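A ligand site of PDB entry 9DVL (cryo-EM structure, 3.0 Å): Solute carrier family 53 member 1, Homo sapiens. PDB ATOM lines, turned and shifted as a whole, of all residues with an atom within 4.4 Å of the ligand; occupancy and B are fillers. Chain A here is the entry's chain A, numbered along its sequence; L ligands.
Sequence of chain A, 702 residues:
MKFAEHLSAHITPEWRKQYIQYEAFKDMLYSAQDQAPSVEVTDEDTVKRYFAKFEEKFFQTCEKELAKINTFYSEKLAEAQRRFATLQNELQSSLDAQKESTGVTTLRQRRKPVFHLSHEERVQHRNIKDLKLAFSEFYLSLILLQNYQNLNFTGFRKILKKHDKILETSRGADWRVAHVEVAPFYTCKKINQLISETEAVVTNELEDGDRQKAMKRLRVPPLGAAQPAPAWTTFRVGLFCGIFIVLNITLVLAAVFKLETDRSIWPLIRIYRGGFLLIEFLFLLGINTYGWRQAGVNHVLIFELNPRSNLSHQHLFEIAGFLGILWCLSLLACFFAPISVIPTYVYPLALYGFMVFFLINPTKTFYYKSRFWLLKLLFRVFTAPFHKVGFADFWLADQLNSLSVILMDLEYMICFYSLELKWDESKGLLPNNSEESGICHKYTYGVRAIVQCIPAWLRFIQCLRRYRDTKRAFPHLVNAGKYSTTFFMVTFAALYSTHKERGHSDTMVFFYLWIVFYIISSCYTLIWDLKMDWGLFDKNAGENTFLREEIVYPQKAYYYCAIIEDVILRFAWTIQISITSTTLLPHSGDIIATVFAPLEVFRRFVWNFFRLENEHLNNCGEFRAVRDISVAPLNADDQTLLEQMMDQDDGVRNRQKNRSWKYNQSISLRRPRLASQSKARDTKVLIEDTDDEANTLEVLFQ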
ATOM      1  N   LEU A 278     -16.308 -17.750 -15.929  1.00  0.00           N
ATOM      2  CA  LEU A 278     -15.721 -18.122 -17.215  1.00  0.00           C
ATOM      3  C   LEU A 278     -16.421 -19.336 -17.807  1.00  0.00           C
ATOM      4  O   LEU A 278     -16.729 -19.375 -19.006  1.00  0.00           O
ATOM      5  CB  LEU A 278     -14.221 -18.387 -17.051  1.00  0.00           C
ATOM      6  CG  LEU A 278     -13.431 -18.628 -18.336  1.00  0.00           C
ATOM      7  CD1 LEU A 278     -12.809 -17.326 -18.829  1.00  0.00           C
ATOM      8  CD2 LEU A 278     -12.376 -19.693 -18.118  1.00  0.00           C
ATOM      9  N   PHE A 281     -19.835 -18.343 -19.042  1.00  0.00           N
ATOM     10  CA  PHE A 281     -19.714 -17.580 -20.278  1.00  0.00           C
ATOM     11  C   PHE A 281     -19.445 -18.504 -21.456  1.00  0.00           C
ATOM     12  O   PHE A 281     -20.000 -18.307 -22.545  1.00  0.00           O
ATOM     13  CB  PHE A 281     -18.616 -16.528 -20.153  1.00  0.00           C
ATOM     14  CG  PHE A 281     -18.316 -15.805 -21.427  1.00  0.00           C
ATOM     15  CD1 PHE A 281     -19.075 -14.721 -21.830  1.00  0.00           C
ATOM     16  CD2 PHE A 281     -17.258 -16.212 -22.234  1.00  0.00           C
ATOM     17  CE1 PHE A 281     -18.798 -14.062 -23.002  1.00  0.00           C
ATOM     18  CE2 PHE A 281     -16.977 -15.543 -23.417  1.00  0.00           C
ATOM     19  CZ  PHE A 281     -17.752 -14.468 -23.802  1.00  0.00           C
ATOM     20  N   LEU A 282     -18.585 -19.504 -21.280  1.00  0.00           N
ATOM     21  CA  LEU A 282     -18.305 -20.434 -22.360  1.00  0.00           C
ATOM     22  C   LEU A 282     -19.554 -21.223 -22.757  1.00  0.00           C
ATOM     23  O   LEU A 282     -19.827 -21.413 -23.946  1.00  0.00           O
ATOM     24  CB  LEU A 282     -17.173 -21.383 -21.970  1.00  0.00           C
ATOM     25  CG  LEU A 282     -15.762 -20.786 -22.056  1.00  0.00           C
ATOM     26  CD1 LEU A 282     -14.758 -21.663 -21.342  1.00  0.00           C
ATOM     27  CD2 LEU A 282     -15.348 -20.578 -23.514  1.00  0.00           C
ATOM     28  N   LEU A 285     -21.809 -19.019 -24.612  1.00  0.00           N
ATOM     29  CA  LEU A 285     -21.257 -18.739 -25.929  1.00  0.00           C
ATOM     30  C   LEU A 285     -21.553 -19.889 -26.885  1.00  0.00           C
ATOM     31  O   LEU A 285     -21.849 -19.657 -28.066  1.00  0.00           O
ATOM     32  CB  LEU A 285     -19.756 -18.497 -25.828  1.00  0.00           C
ATOM     33  CG  LEU A 285     -19.210 -17.060 -25.883  1.00  0.00           C
ATOM     34  CD1 LEU A 285     -17.778 -17.085 -26.372  1.00  0.00           C
ATOM     35  CD2 LEU A 285     -20.049 -16.137 -26.759  1.00  0.00           C
ATOM     36  N   THR A 289     -23.673 -19.566 -30.324  1.00  0.00           N
ATOM     37  CA  THR A 289     -23.283 -20.091 -31.627  1.00  0.00           C
ATOM     38  C   THR A 289     -24.377 -20.976 -32.202  1.00  0.00           C
ATOM     39  O   THR A 289     -24.704 -20.884 -33.394  1.00  0.00           O
ATOM     40  CB  THR A 289     -21.967 -20.852 -31.518  1.00  0.00           C
ATOM     41  OG1 THR A 289     -21.026 -20.081 -30.762  1.00  0.00           O
ATOM     42  CG2 THR A 289     -21.392 -21.148 -32.896  1.00  0.00           C
ATOM     43  N   TRP A 292     -27.231 -18.722 -33.382  1.00  0.00           N
ATOM     44  CA  TRP A 292     -26.866 -17.998 -34.595  1.00  0.00           C
ATOM     45  C   TRP A 292     -26.931 -18.920 -35.810  1.00  0.00           C
ATOM     46  O   TRP A 292     -27.426 -18.533 -36.873  1.00  0.00           O
ATOM     47  CB  TRP A 292     -25.468 -17.399 -34.465  1.00  0.00           C
ATOM     48  CG  TRP A 292     -25.375 -16.307 -33.430  1.00  0.00           C
ATOM     49  CD1 TRP A 292     -26.350 -15.435 -33.067  1.00  0.00           C
ATOM     50  CD2 TRP A 292     -24.228 -15.994 -32.635  1.00  0.00           C
ATOM     51  NE1 TRP A 292     -25.889 -14.593 -32.094  1.00  0.00           N
ATOM     52  CE2 TRP A 292     -24.584 -14.904 -31.808  1.00  0.00           C
ATOM     53  CE3 TRP A 292     -22.934 -16.515 -32.537  1.00  0.00           C
ATOM     54  CZ2 TRP A 292     -23.695 -14.343 -30.897  1.00  0.00           C
ATOM     55  CZ3 TRP A 292     -22.053 -15.944 -31.630  1.00  0.00           C
ATOM     56  CH2 TRP A 292     -22.436 -14.873 -30.820  1.00  0.00           C
ATOM     57  N   PHE A 303     -17.901 -11.998 -37.594  1.00  0.00           N
ATOM     58  CA  PHE A 303     -16.635 -12.115 -36.883  1.00  0.00           C
ATOM     59  C   PHE A 303     -15.446 -12.264 -37.824  1.00  0.00           C
ATOM     60  O   PHE A 303     -14.308 -12.327 -37.342  1.00  0.00           O
ATOM     61  CB  PHE A 303     -16.674 -13.317 -35.928  1.00  0.00           C
ATOM     62  CG  PHE A 303     -17.427 -13.038 -34.655  1.00  0.00           C
ATOM     63  CD1 PHE A 303     -16.861 -12.259 -33.656  1.00  0.00           C
ATOM     64  CD2 PHE A 303     -18.695 -13.565 -34.447  1.00  0.00           C
ATOM     65  CE1 PHE A 303     -17.542 -12.009 -32.486  1.00  0.00           C
ATOM     66  CE2 PHE A 303     -19.376 -13.316 -33.276  1.00  0.00           C
ATOM     67  CZ  PHE A 303     -18.807 -12.537 -32.287  1.00  0.00           C
ATOM     68  N   LEU A 305     -14.467 -14.781 -39.387  1.00  0.00           N
ATOM     69  CA  LEU A 305     -13.825 -16.072 -39.205  1.00  0.00           C
ATOM     70  C   LEU A 305     -13.737 -16.816 -40.532  1.00  0.00           C
ATOM     71  O   LEU A 305     -14.519 -16.580 -41.452  1.00  0.00           O
ATOM     72  CB  LEU A 305     -14.593 -16.919 -38.188  1.00  0.00           C
ATOM     73  CG  LEU A 305     -14.924 -16.225 -36.858  1.00  0.00           C
ATOM     74  CD1 LEU A 305     -16.091 -16.912 -36.170  1.00  0.00           C
ATOM     75  CD2 LEU A 305     -13.700 -16.190 -35.959  1.00  0.00           C
ATOM     76  N   ASN A 306     -12.772 -17.723 -40.624  1.00  0.00           N
ATOM     77  CA  ASN A 306     -12.574 -18.496 -41.833  1.00  0.00           C
ATOM     78  C   ASN A 306     -13.770 -19.410 -42.070  1.00  0.00           C
ATOM     79  O   ASN A 306     -14.112 -20.201 -41.180  1.00  0.00           O
ATOM     80  CB  ASN A 306     -11.297 -19.317 -41.741  1.00  0.00           C
ATOM     81  CG  ASN A 306     -10.892 -19.934 -43.066  1.00  0.00           C
ATOM     82  OD1 ASN A 306     -11.606 -20.774 -43.613  1.00  0.00           O
ATOM     83  ND2 ASN A 306      -9.743 -19.518 -43.584  1.00  0.00           N
ATOM     84  N   SER A 309     -13.094 -23.376 -41.476  1.00  0.00           N
ATOM     85  CA  SER A 309     -12.914 -23.824 -40.106  1.00  0.00           C
ATOM     86  C   SER A 309     -13.785 -22.988 -39.187  1.00  0.00           C
ATOM     87  O   SER A 309     -13.599 -21.768 -39.074  1.00  0.00           O
ATOM     88  CB  SER A 309     -11.447 -23.725 -39.693  1.00  0.00           C
ATOM     89  OG  SER A 309     -10.856 -22.543 -40.198  1.00  0.00           O
ATOM     90  N   ASN A 310     -14.745 -23.635 -38.523  1.00  0.00           N
ATOM     91  CA  ASN A 310     -15.630 -22.977 -37.576  1.00  0.00           C
ATOM     92  C   ASN A 310     -15.756 -23.840 -36.334  1.00  0.00           C
ATOM     93  O   ASN A 310     -15.875 -25.062 -36.427  1.00  0.00           O
ATOM     94  CB  ASN A 310     -17.019 -22.729 -38.176  1.00  0.00           C
ATOM     95  CG  ASN A 310     -16.966 -21.915 -39.458  1.00  0.00           C
ATOM     96  OD1 ASN A 310     -16.086 -21.070 -39.635  1.00  0.00           O
ATOM     97  ND2 ASN A 310     -17.900 -22.174 -40.369  1.00  0.00           N
ATOM     98  N   LEU A 311     -15.736 -23.199 -35.167  1.00  0.00           N
ATOM     99  CA  LEU A 311     -15.915 -23.908 -33.909  1.00  0.00           C
ATOM    100  C   LEU A 311     -17.402 -24.071 -33.634  1.00  0.00           C
ATOM    101  O   LEU A 311     -18.138 -23.083 -33.531  1.00  0.00           O
ATOM    102  CB  LEU A 311     -15.235 -23.146 -32.771  1.00  0.00           C
ATOM    103  CG  LEU A 311     -15.203 -23.869 -31.417  1.00  0.00           C
ATOM    104  CD1 LEU A 311     -14.259 -25.064 -31.465  1.00  0.00           C
ATOM    105  CD2 LEU A 311     -14.801 -22.917 -30.312  1.00  0.00           C
ATOM    106  N   LEU A 316     -17.646 -25.823 -27.788  1.00  0.00           N
ATOM    107  CA  LEU A 316     -17.687 -24.882 -26.669  1.00  0.00           C
ATOM    108  C   LEU A 316     -18.305 -25.534 -25.442  1.00  0.00           C
ATOM    109  O   LEU A 316     -17.824 -25.326 -24.317  1.00  0.00           O
ATOM    110  CB  LEU A 316     -18.471 -23.637 -27.078  1.00  0.00           C
ATOM    111  CG  LEU A 316     -17.702 -22.600 -27.908  1.00  0.00           C
ATOM    112  CD1 LEU A 316     -18.655 -21.610 -28.540  1.00  0.00           C
ATOM    113  CD2 LEU A 316     -16.677 -21.877 -27.051  1.00  0.00           C
ATOM    114  N   ILE A 319     -15.655 -27.771 -23.896  1.00  0.00           N
ATOM    115  CA  ILE A 319     -14.639 -27.015 -23.179  1.00  0.00           C
ATOM    116  C   ILE A 319     -15.197 -26.521 -21.841  1.00  0.00           C
ATOM    117  O   ILE A 319     -14.533 -26.636 -20.797  1.00  0.00           O
ATOM    118  CB  ILE A 319     -14.140 -25.838 -24.036  1.00  0.00           C
ATOM    119  CG1 ILE A 319     -13.527 -26.332 -25.348  1.00  0.00           C
ATOM    120  CG2 ILE A 319     -13.119 -25.019 -23.260  1.00  0.00           C
ATOM    121  CD1 ILE A 319     -13.622 -25.324 -26.466  1.00  0.00           C
ATOM    122  N   MET A 355      -5.915 -23.443 -16.732  1.00  0.00           N
ATOM    123  CA  MET A 355      -6.698 -22.636 -17.668  1.00  0.00           C
ATOM    124  C   MET A 355      -5.776 -21.746 -18.495  1.00  0.00           C
ATOM    125  O   MET A 355      -5.842 -21.727 -19.729  1.00  0.00           O
ATOM    126  CB  MET A 355      -7.719 -21.792 -16.910  1.00  0.00           C
ATOM    127  CG  MET A 355      -9.073 -22.458 -16.740  1.00  0.00           C
ATOM    128  SD  MET A 355     -10.215 -21.458 -15.776  1.00  0.00           S
ATOM    129  CE  MET A 355     -11.527 -22.638 -15.446  1.00  0.00           C
ATOM    130  N   VAL A 356      -4.874 -21.028 -17.820  1.00  0.00           N
ATOM    131  CA  VAL A 356      -3.935 -20.172 -18.535  1.00  0.00           C
ATOM    132  C   VAL A 356      -3.126 -21.009 -19.525  1.00  0.00           C
ATOM    133  O   VAL A 356      -3.041 -20.693 -20.713  1.00  0.00           O
ATOM    134  CB  VAL A 356      -3.023 -19.428 -17.546  1.00  0.00           C
ATOM    135  CG1 VAL A 356      -1.668 -19.106 -18.164  1.00  0.00           C
ATOM    136  CG2 VAL A 356      -3.711 -18.161 -17.060  1.00  0.00           C
ATOM    137  N   PHE A 358      -3.964 -23.742 -20.730  1.00  0.00           N
ATOM    138  CA  PHE A 358      -4.862 -24.209 -21.775  1.00  0.00           C
ATOM    139  C   PHE A 358      -5.028 -23.156 -22.866  1.00  0.00           C
ATOM    140  O   PHE A 358      -5.139 -23.493 -24.049  1.00  0.00           O
ATOM    141  CB  PHE A 358      -6.214 -24.582 -21.174  1.00  0.00           C
ATOM    142  CG  PHE A 358      -7.191 -25.144 -22.174  1.00  0.00           C
ATOM    143  CD1 PHE A 358      -7.152 -26.486 -22.525  1.00  0.00           C
ATOM    144  CD2 PHE A 358      -8.139 -24.333 -22.772  1.00  0.00           C
ATOM    145  CE1 PHE A 358      -8.037 -26.998 -23.448  1.00  0.00           C
ATOM    146  CE2 PHE A 358      -9.033 -24.844 -23.697  1.00  0.00           C
ATOM    147  CZ  PHE A 358      -8.987 -26.176 -24.037  1.00  0.00           C
ATOM    148  N   LEU A 359      -5.049 -21.882 -22.473  1.00  0.00           N
ATOM    149  CA  LEU A 359      -5.239 -20.812 -23.446  1.00  0.00           C
ATOM    150  C   LEU A 359      -3.968 -20.546 -24.243  1.00  0.00           C
ATOM    151  O   LEU A 359      -4.036 -20.305 -25.450  1.00  0.00           O
ATOM    152  CB  LEU A 359      -5.705 -19.542 -22.726  1.00  0.00           C
ATOM    153  CG  LEU A 359      -5.589 -18.213 -23.478  1.00  0.00           C
ATOM    154  CD1 LEU A 359      -6.580 -18.130 -24.618  1.00  0.00           C
ATOM    155  CD2 LEU A 359      -5.786 -17.052 -22.513  1.00  0.00           C
ATOM    156  N   LYS A 369      -6.079 -23.384 -33.355  1.00  0.00           N
ATOM    157  CA  LYS A 369      -6.326 -22.246 -34.235  1.00  0.00           C
ATOM    158  C   LYS A 369      -7.239 -21.231 -33.580  1.00  0.00           C
ATOM    159  O   LYS A 369      -6.948 -20.020 -33.571  1.00  0.00           O
ATOM    160  CB  LYS A 369      -6.923 -22.740 -35.554  1.00  0.00           C
ATOM    161  CG  LYS A 369      -6.094 -23.823 -36.250  1.00  0.00           C
ATOM    162  CD  LYS A 369      -6.829 -24.435 -37.435  1.00  0.00           C
ATOM    163  CE  LYS A 369      -7.296 -23.384 -38.427  1.00  0.00           C
ATOM    164  NZ  LYS A 369      -6.230 -22.394 -38.757  1.00  0.00           N
ATOM    165  N   SER A 370      -8.351 -21.696 -33.016  1.00  0.00           N
ATOM    166  CA  SER A 370      -9.284 -20.790 -32.339  1.00  0.00           C
ATOM    167  C   SER A 370      -8.629 -20.144 -31.128  1.00  0.00           C
ATOM    168  O   SER A 370      -8.863 -18.966 -30.835  1.00  0.00           O
ATOM    169  CB  SER A 370     -10.553 -21.538 -31.940  1.00  0.00           C
ATOM    170  OG  SER A 370     -10.424 -22.108 -30.651  1.00  0.00           O
ATOM    171  N   ARG A 371      -7.815 -20.902 -30.395  1.00  0.00           N
ATOM    172  CA  ARG A 371      -7.140 -20.349 -29.224  1.00  0.00           C
ATOM    173  C   ARG A 371      -6.172 -19.238 -29.633  1.00  0.00           C
ATOM    174  O   ARG A 371      -6.104 -18.195 -28.969  1.00  0.00           O
ATOM    175  CB  ARG A 371      -6.404 -21.454 -28.472  1.00  0.00           C
ATOM    176  CG  ARG A 371      -7.317 -22.366 -27.673  1.00  0.00           C
ATOM    177  CD  ARG A 371      -6.523 -23.274 -26.748  1.00  0.00           C
ATOM    178  NE  ARG A 371      -5.583 -24.113 -27.479  1.00  0.00           N
ATOM    179  CZ  ARG A 371      -4.284 -23.854 -27.608  1.00  0.00           C
ATOM    180  NH1 ARG A 371      -3.734 -22.778 -27.083  1.00  0.00           N
ATOM    181  NH2 ARG A 371      -3.523 -24.703 -28.298  1.00  0.00           N
ATOM    182  N   TRP A 373      -6.393 -17.386 -32.371  1.00  0.00           N
ATOM    183  CA  TRP A 373      -7.208 -16.261 -32.793  1.00  0.00           C
ATOM    184  C   TRP A 373      -7.719 -15.475 -31.584  1.00  0.00           C
ATOM    185  O   TRP A 373      -7.705 -14.233 -31.587  1.00  0.00           O
ATOM    186  CB  TRP A 373      -8.371 -16.737 -33.655  1.00  0.00           C
ATOM    187  CG  TRP A 373      -9.273 -15.632 -34.133  1.00  0.00           C
ATOM    188  CD1 TRP A 373      -9.077 -14.845 -35.233  1.00  0.00           C
ATOM    189  CD2 TRP A 373     -10.495 -15.199 -33.544  1.00  0.00           C
ATOM    190  NE1 TRP A 373     -10.102 -13.946 -35.358  1.00  0.00           N
ATOM    191  CE2 TRP A 373     -10.993 -14.146 -34.326  1.00  0.00           C
ATOM    192  CE3 TRP A 373     -11.231 -15.610 -32.421  1.00  0.00           C
ATOM    193  CZ2 TRP A 373     -12.182 -13.489 -34.035  1.00  0.00           C
ATOM    194  CZ3 TRP A 373     -12.410 -14.954 -32.126  1.00  0.00           C
ATOM    195  CH2 TRP A 373     -12.881 -13.903 -32.932  1.00  0.00           C
ATOM    196  N   LEU A 374      -8.167 -16.184 -30.543  1.00  0.00           N
ATOM    197  CA  LEU A 374      -8.619 -15.521 -29.331  1.00  0.00           C
ATOM    198  C   LEU A 374      -7.493 -14.753 -28.666  1.00  0.00           C
ATOM    199  O   LEU A 374      -7.687 -13.636 -28.168  1.00  0.00           O
ATOM    200  CB  LEU A 374      -9.217 -16.549 -28.377  1.00  0.00           C
ATOM    201  CG  LEU A 374      -9.426 -16.114 -26.919  1.00  0.00           C
ATOM    202  CD1 LEU A 374     -10.264 -14.851 -26.834  1.00  0.00           C
ATOM    203  CD2 LEU A 374     -10.063 -17.238 -26.118  1.00  0.00           C
ATOM    204  N   LEU A 378      -7.542 -10.778 -28.016  1.00  0.00           N
ATOM    205  CA  LEU A 378      -7.365 -10.206 -26.682  1.00  0.00           C
ATOM    206  C   LEU A 378      -6.212  -9.202 -26.672  1.00  0.00           C
ATOM    207  O   LEU A 378      -6.338  -8.114 -26.090  1.00  0.00           O
ATOM    208  CB  LEU A 378      -7.106 -11.316 -25.664  1.00  0.00           C
ATOM    209  CG  LEU A 378      -8.304 -12.177 -25.267  1.00  0.00           C
ATOM    210  CD1 LEU A 378      -7.845 -13.581 -24.903  1.00  0.00           C
ATOM    211  CD2 LEU A 378      -9.064 -11.544 -24.113  1.00  0.00           C
ATOM    212  N   TRP A 395     -16.665  -6.516 -29.815  1.00  0.00           N
ATOM    213  CA  TRP A 395     -17.455  -7.552 -29.159  1.00  0.00           C
ATOM    214  C   TRP A 395     -16.720  -8.153 -27.979  1.00  0.00           C
ATOM    215  O   TRP A 395     -17.293  -8.343 -26.894  1.00  0.00           O
ATOM    216  CB  TRP A 395     -17.832  -8.621 -30.186  1.00  0.00           C
ATOM    217  CG  TRP A 395     -18.647  -9.740 -29.627  1.00  0.00           C
ATOM    218  CD1 TRP A 395     -20.004  -9.810 -29.569  1.00  0.00           C
ATOM    219  CD2 TRP A 395     -18.155 -10.954 -29.045  1.00  0.00           C
ATOM    220  NE1 TRP A 395     -20.388 -10.997 -28.991  1.00  0.00           N
ATOM    221  CE2 TRP A 395     -19.273 -11.708 -28.663  1.00  0.00           C
ATOM    222  CE3 TRP A 395     -16.869 -11.467 -28.815  1.00  0.00           C
ATOM    223  CZ2 TRP A 395     -19.145 -12.955 -28.052  1.00  0.00           C
ATOM    224  CZ3 TRP A 395     -16.748 -12.704 -28.217  1.00  0.00           C
ATOM    225  CH2 TRP A 395     -17.884 -13.429 -27.842  1.00  0.00           C
ATOM    226  N   LEU A 396     -15.433  -8.457 -28.149  1.00  0.00           N
ATOM    227  CA  LEU A 396     -14.651  -9.024 -27.051  1.00  0.00           C
ATOM    228  C   LEU A 396     -14.461  -8.002 -25.930  1.00  0.00           C
ATOM    229  O   LEU A 396     -14.459  -8.373 -24.755  1.00  0.00           O
ATOM    230  CB  LEU A 396     -13.293  -9.500 -27.575  1.00  0.00           C
ATOM    231  CG  LEU A 396     -12.420 -10.256 -26.553  1.00  0.00           C
ATOM    232  CD1 LEU A 396     -13.002 -11.630 -26.273  1.00  0.00           C
ATOM    233  CD2 LEU A 396     -10.996 -10.362 -27.060  1.00  0.00           C
ATOM    234  N   LEU A 400     -15.549  -8.528 -22.059  1.00  0.00           N
ATOM    235  CA  LEU A 400     -14.729  -8.192 -20.904  1.00  0.00           C
ATOM    236  C   LEU A 400     -15.465  -7.241 -19.973  1.00  0.00           C
ATOM    237  O   LEU A 400     -15.402  -7.390 -18.741  1.00  0.00           O
ATOM    238  CB  LEU A 400     -13.398  -7.590 -21.349  1.00  0.00           C
ATOM    239  CG  LEU A 400     -12.478  -8.492 -22.155  1.00  0.00           C
ATOM    240  CD1 LEU A 400     -11.330  -7.699 -22.740  1.00  0.00           C
ATOM    241  CD2 LEU A 400     -11.963  -9.642 -21.298  1.00  0.00           C
ATOM    242  N   ILE A 406     -14.207 -10.710 -12.572  1.00  0.00           N
ATOM    243  CA  ILE A 406     -13.030 -11.568 -12.499  1.00  0.00           C
ATOM    244  C   ILE A 406     -11.791 -10.741 -12.169  1.00  0.00           C
ATOM    245  O   ILE A 406     -10.987 -11.111 -11.298  1.00  0.00           O
ATOM    246  CB  ILE A 406     -12.851 -12.345 -13.818  1.00  0.00           C
ATOM    247  CG1 ILE A 406     -14.162 -13.003 -14.242  1.00  0.00           C
ATOM    248  CG2 ILE A 406     -11.753 -13.386 -13.672  1.00  0.00           C
ATOM    249  CD1 ILE A 406     -14.060 -13.825 -15.518  1.00  0.00           C
ATOM    250  N   LEU A 407     -11.628  -9.611 -12.852  1.00  0.00           N
ATOM    251  CA  LEU A 407     -10.498  -8.732 -12.570  1.00  0.00           C
ATOM    252  C   LEU A 407     -10.567  -8.175 -11.151  1.00  0.00           C
ATOM    253  O   LEU A 407      -9.552  -8.081 -10.455  1.00  0.00           O
ATOM    254  CB  LEU A 407     -10.442  -7.594 -13.589  1.00  0.00           C
ATOM    255  CG  LEU A 407      -9.497  -7.796 -14.767  1.00  0.00           C
ATOM    256  CD1 LEU A 407      -9.821  -9.093 -15.503  1.00  0.00           C
ATOM    257  CD2 LEU A 407      -9.554  -6.610 -15.718  1.00  0.00           C
HETATM  258  C1  LIG L   1     -14.823 -19.630 -34.411  1.00  0.00           C
HETATM  259  C2  LIG L   1     -15.425 -19.135 -33.065  1.00  0.00           C
HETATM  260  C3  LIG L   1     -14.347 -18.242 -32.370  1.00  0.00           C
HETATM  261  C4  LIG L   1     -11.350 -19.097 -35.590  1.00  0.00           C
HETATM  262  C5  LIG L   1     -10.045 -19.764 -35.992  1.00  0.00           C
HETATM  263  C6  LIG L   1      -9.785 -17.707 -37.469  1.00  0.00           C
HETATM  264  C7  LIG L   1     -10.555 -19.895 -38.364  1.00  0.00           C
HETATM  265  C8  LIG L   1      -8.202 -19.609 -37.687  1.00  0.00           C
HETATM  266  C9  LIG L   1     -12.728 -18.725 -30.682  1.00  0.00           C
HETATM  267  C10 LIG L   1     -12.639 -19.818 -29.654  1.00  0.00           C
HETATM  268  C11 LIG L   1     -13.807 -19.746 -28.649  1.00  0.00           C
HETATM  269  C12 LIG L   1     -13.385 -20.020 -27.197  1.00  0.00           C
HETATM  270  C13 LIG L   1     -12.916 -21.470 -26.942  1.00  0.00           C
HETATM  271  C14 LIG L   1     -12.163 -21.623 -25.608  1.00  0.00           C
HETATM  272  C15 LIG L   1     -10.675 -21.238 -25.657  1.00  0.00           C
HETATM  273  C16 LIG L   1      -9.975 -21.326 -24.280  1.00  0.00           C
HETATM  274  C17 LIG L   1     -10.274 -20.180 -23.293  1.00  0.00           C
HETATM  275  C18 LIG L   1      -9.694 -20.301 -21.866  1.00  0.00           C
HETATM  276  C19 LIG L   1      -9.700 -19.034 -21.008  1.00  0.00           C
HETATM  277  C20 LIG L   1      -8.723 -19.124 -19.820  1.00  0.00           C
HETATM  278  C21 LIG L   1      -8.439 -17.797 -19.120  1.00  0.00           C
HETATM  279  C22 LIG L   1      -7.834 -17.960 -17.714  1.00  0.00           C
HETATM  280  C23 LIG L   1      -7.884 -16.654 -16.913  1.00  0.00           C
HETATM  281  C24 LIG L   1      -7.013 -15.582 -17.558  1.00  0.00           C
HETATM  282  C25 LIG L   1     -17.507 -18.162 -32.246  1.00  0.00           C
HETATM  283  C26 LIG L   1     -17.967 -16.719 -32.048  1.00  0.00           C
HETATM  284  C27 LIG L   1     -16.866 -15.842 -31.429  1.00  0.00           C
HETATM  285  C28 LIG L   1     -16.587 -16.199 -29.963  1.00  0.00           C
HETATM  286  C29 LIG L   1     -15.242 -15.698 -29.455  1.00  0.00           C
HETATM  287  C30 LIG L   1     -15.086 -15.857 -27.944  1.00  0.00           C
HETATM  288  C31 LIG L   1     -13.673 -15.589 -27.412  1.00  0.00           C
HETATM  289  C32 LIG L   1     -13.605 -15.453 -25.894  1.00  0.00           C
HETATM  290  C33 LIG L   1     -13.507 -16.776 -25.225  1.00  0.00           C
HETATM  291  C34 LIG L   1     -12.826 -17.058 -24.113  1.00  0.00           C
HETATM  292  C35 LIG L   1     -12.029 -16.078 -23.310  1.00  0.00           C
HETATM  293  C36 LIG L   1     -12.927 -15.168 -22.539  1.00  0.00           C
HETATM  294  C37 LIG L   1     -12.504 -14.183 -21.744  1.00  0.00           C
HETATM  295  C38 LIG L   1     -11.076 -13.839 -21.494  1.00  0.00           C
HETATM  296  C39 LIG L   1     -10.396 -14.747 -20.468  1.00  0.00           C
HETATM  297  C40 LIG L   1     -10.649 -14.282 -19.036  1.00  0.00           C
HETATM  298  C41 LIG L   1      -9.868 -13.005 -18.706  1.00  0.00           C
HETATM  299  C42 LIG L   1      -9.667 -12.856 -17.212  1.00  0.00           C
HETATM  300  N1  LIG L   1      -9.636 -19.221 -37.368  1.00  0.00           N
HETATM  301  O1  LIG L   1     -16.620 -18.373 -33.264  1.00  0.00           O
HETATM  302  O2  LIG L   1     -13.337 -19.100 -31.845  1.00  0.00           O
HETATM  303  O3  LIG L   1     -12.295 -17.612 -30.529  1.00  0.00           O
HETATM  304  O4  LIG L   1     -17.917 -19.049 -31.517  1.00  0.00           O
HETATM  305  O5  LIG L   1     -12.212 -22.412 -34.515  1.00  0.00           O
HETATM  306  O6  LIG L   1     -13.299 -20.959 -36.567  1.00  0.00           O
HETATM  307  O7  LIG L   1     -14.106 -20.760 -34.155  1.00  0.00           O
HETATM  308  O8  LIG L   1     -11.905 -19.885 -34.617  1.00  0.00           O
HETATM  309  P1  LIG L   1     -12.798 -21.231 -35.207  1.00  0.00           P
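Leu 278 touches the ligand (CD1 to C40, 3.7 Å). Leu 282 touches the ligand (CD2 to C14, 3.95 Å). Leu 285 touches the ligand. CE2 of Phe 303 touches C26 of the ligand, 3.9 Å away. Leu 305 touches the ligand (CD1 to O1, 3.3 Å). Asn 306 touches the ligand (CB to C7, 3.5 Å). Asn 310 touches the ligand (CA to O6, 3.2 Å). Leu 316 touches the ligand (CD2 to C12, 3.8 Å). Ile 319 touches the ligand (CD1 to C13, 3.9 Å). Met 355 touches the ligand. CE2 of Phe 358 touches C16 of the ligand, 3.7 Å away. Lys 369 touches the ligand. Ser 370 touches the ligand. Trp 373 touches the ligand. Leu 374 touches the ligand (CD2 to C34, 3.4 Å). CZ3 of Trp 395 touches C29 of the ligand, at 3.6 Å. Leu 396 touches the ligand (CD1 to C32, 3.9 Å). Hydrophobic or aromatic side chains within 4 Å of the ligand: Leu 278, Leu 282, Leu 285, Phe 303, Leu 305, Leu 311, Leu 316, Ile 319, Met 355, Phe 358, Trp 373, Leu 374, Trp 395 and Leu 396. 20 residues have an atom within 4 Å of the ligand: Leu 278, Leu 282, Leu 285, Thr 289, Phe 303, Leu 305, Asn 306, Ser 309, Asn 310, Leu 311, Leu 316, Ile 319, Met 355, Phe 358, Lys 369, Ser 370, Trp 373, Leu 374, Trp 395 and Leu 396.
The side-chain amide oxygen (OD1) of Asn 310 lies close to the backbone carbonyl oxygen (O) of Asn 306 (2.7 Å). OG1 of Thr 289 sits at hydrogen-bond distance from O of Leu 285, 2.9 Å away. The guanidinium group (NH1) of Arg 371 sits close to the backbone carbonyl oxygen (O) of Phe 358 (3.4 Å).
N of Leu 311 lies close to O7 of the ligand, at 3.1 Å. O4 of the ligand is in hydrogen-bond range of OG1 of Thr 289 (3.4 Å). O6 of the ligand sits close to O of Ser 309 (2.7 Å).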
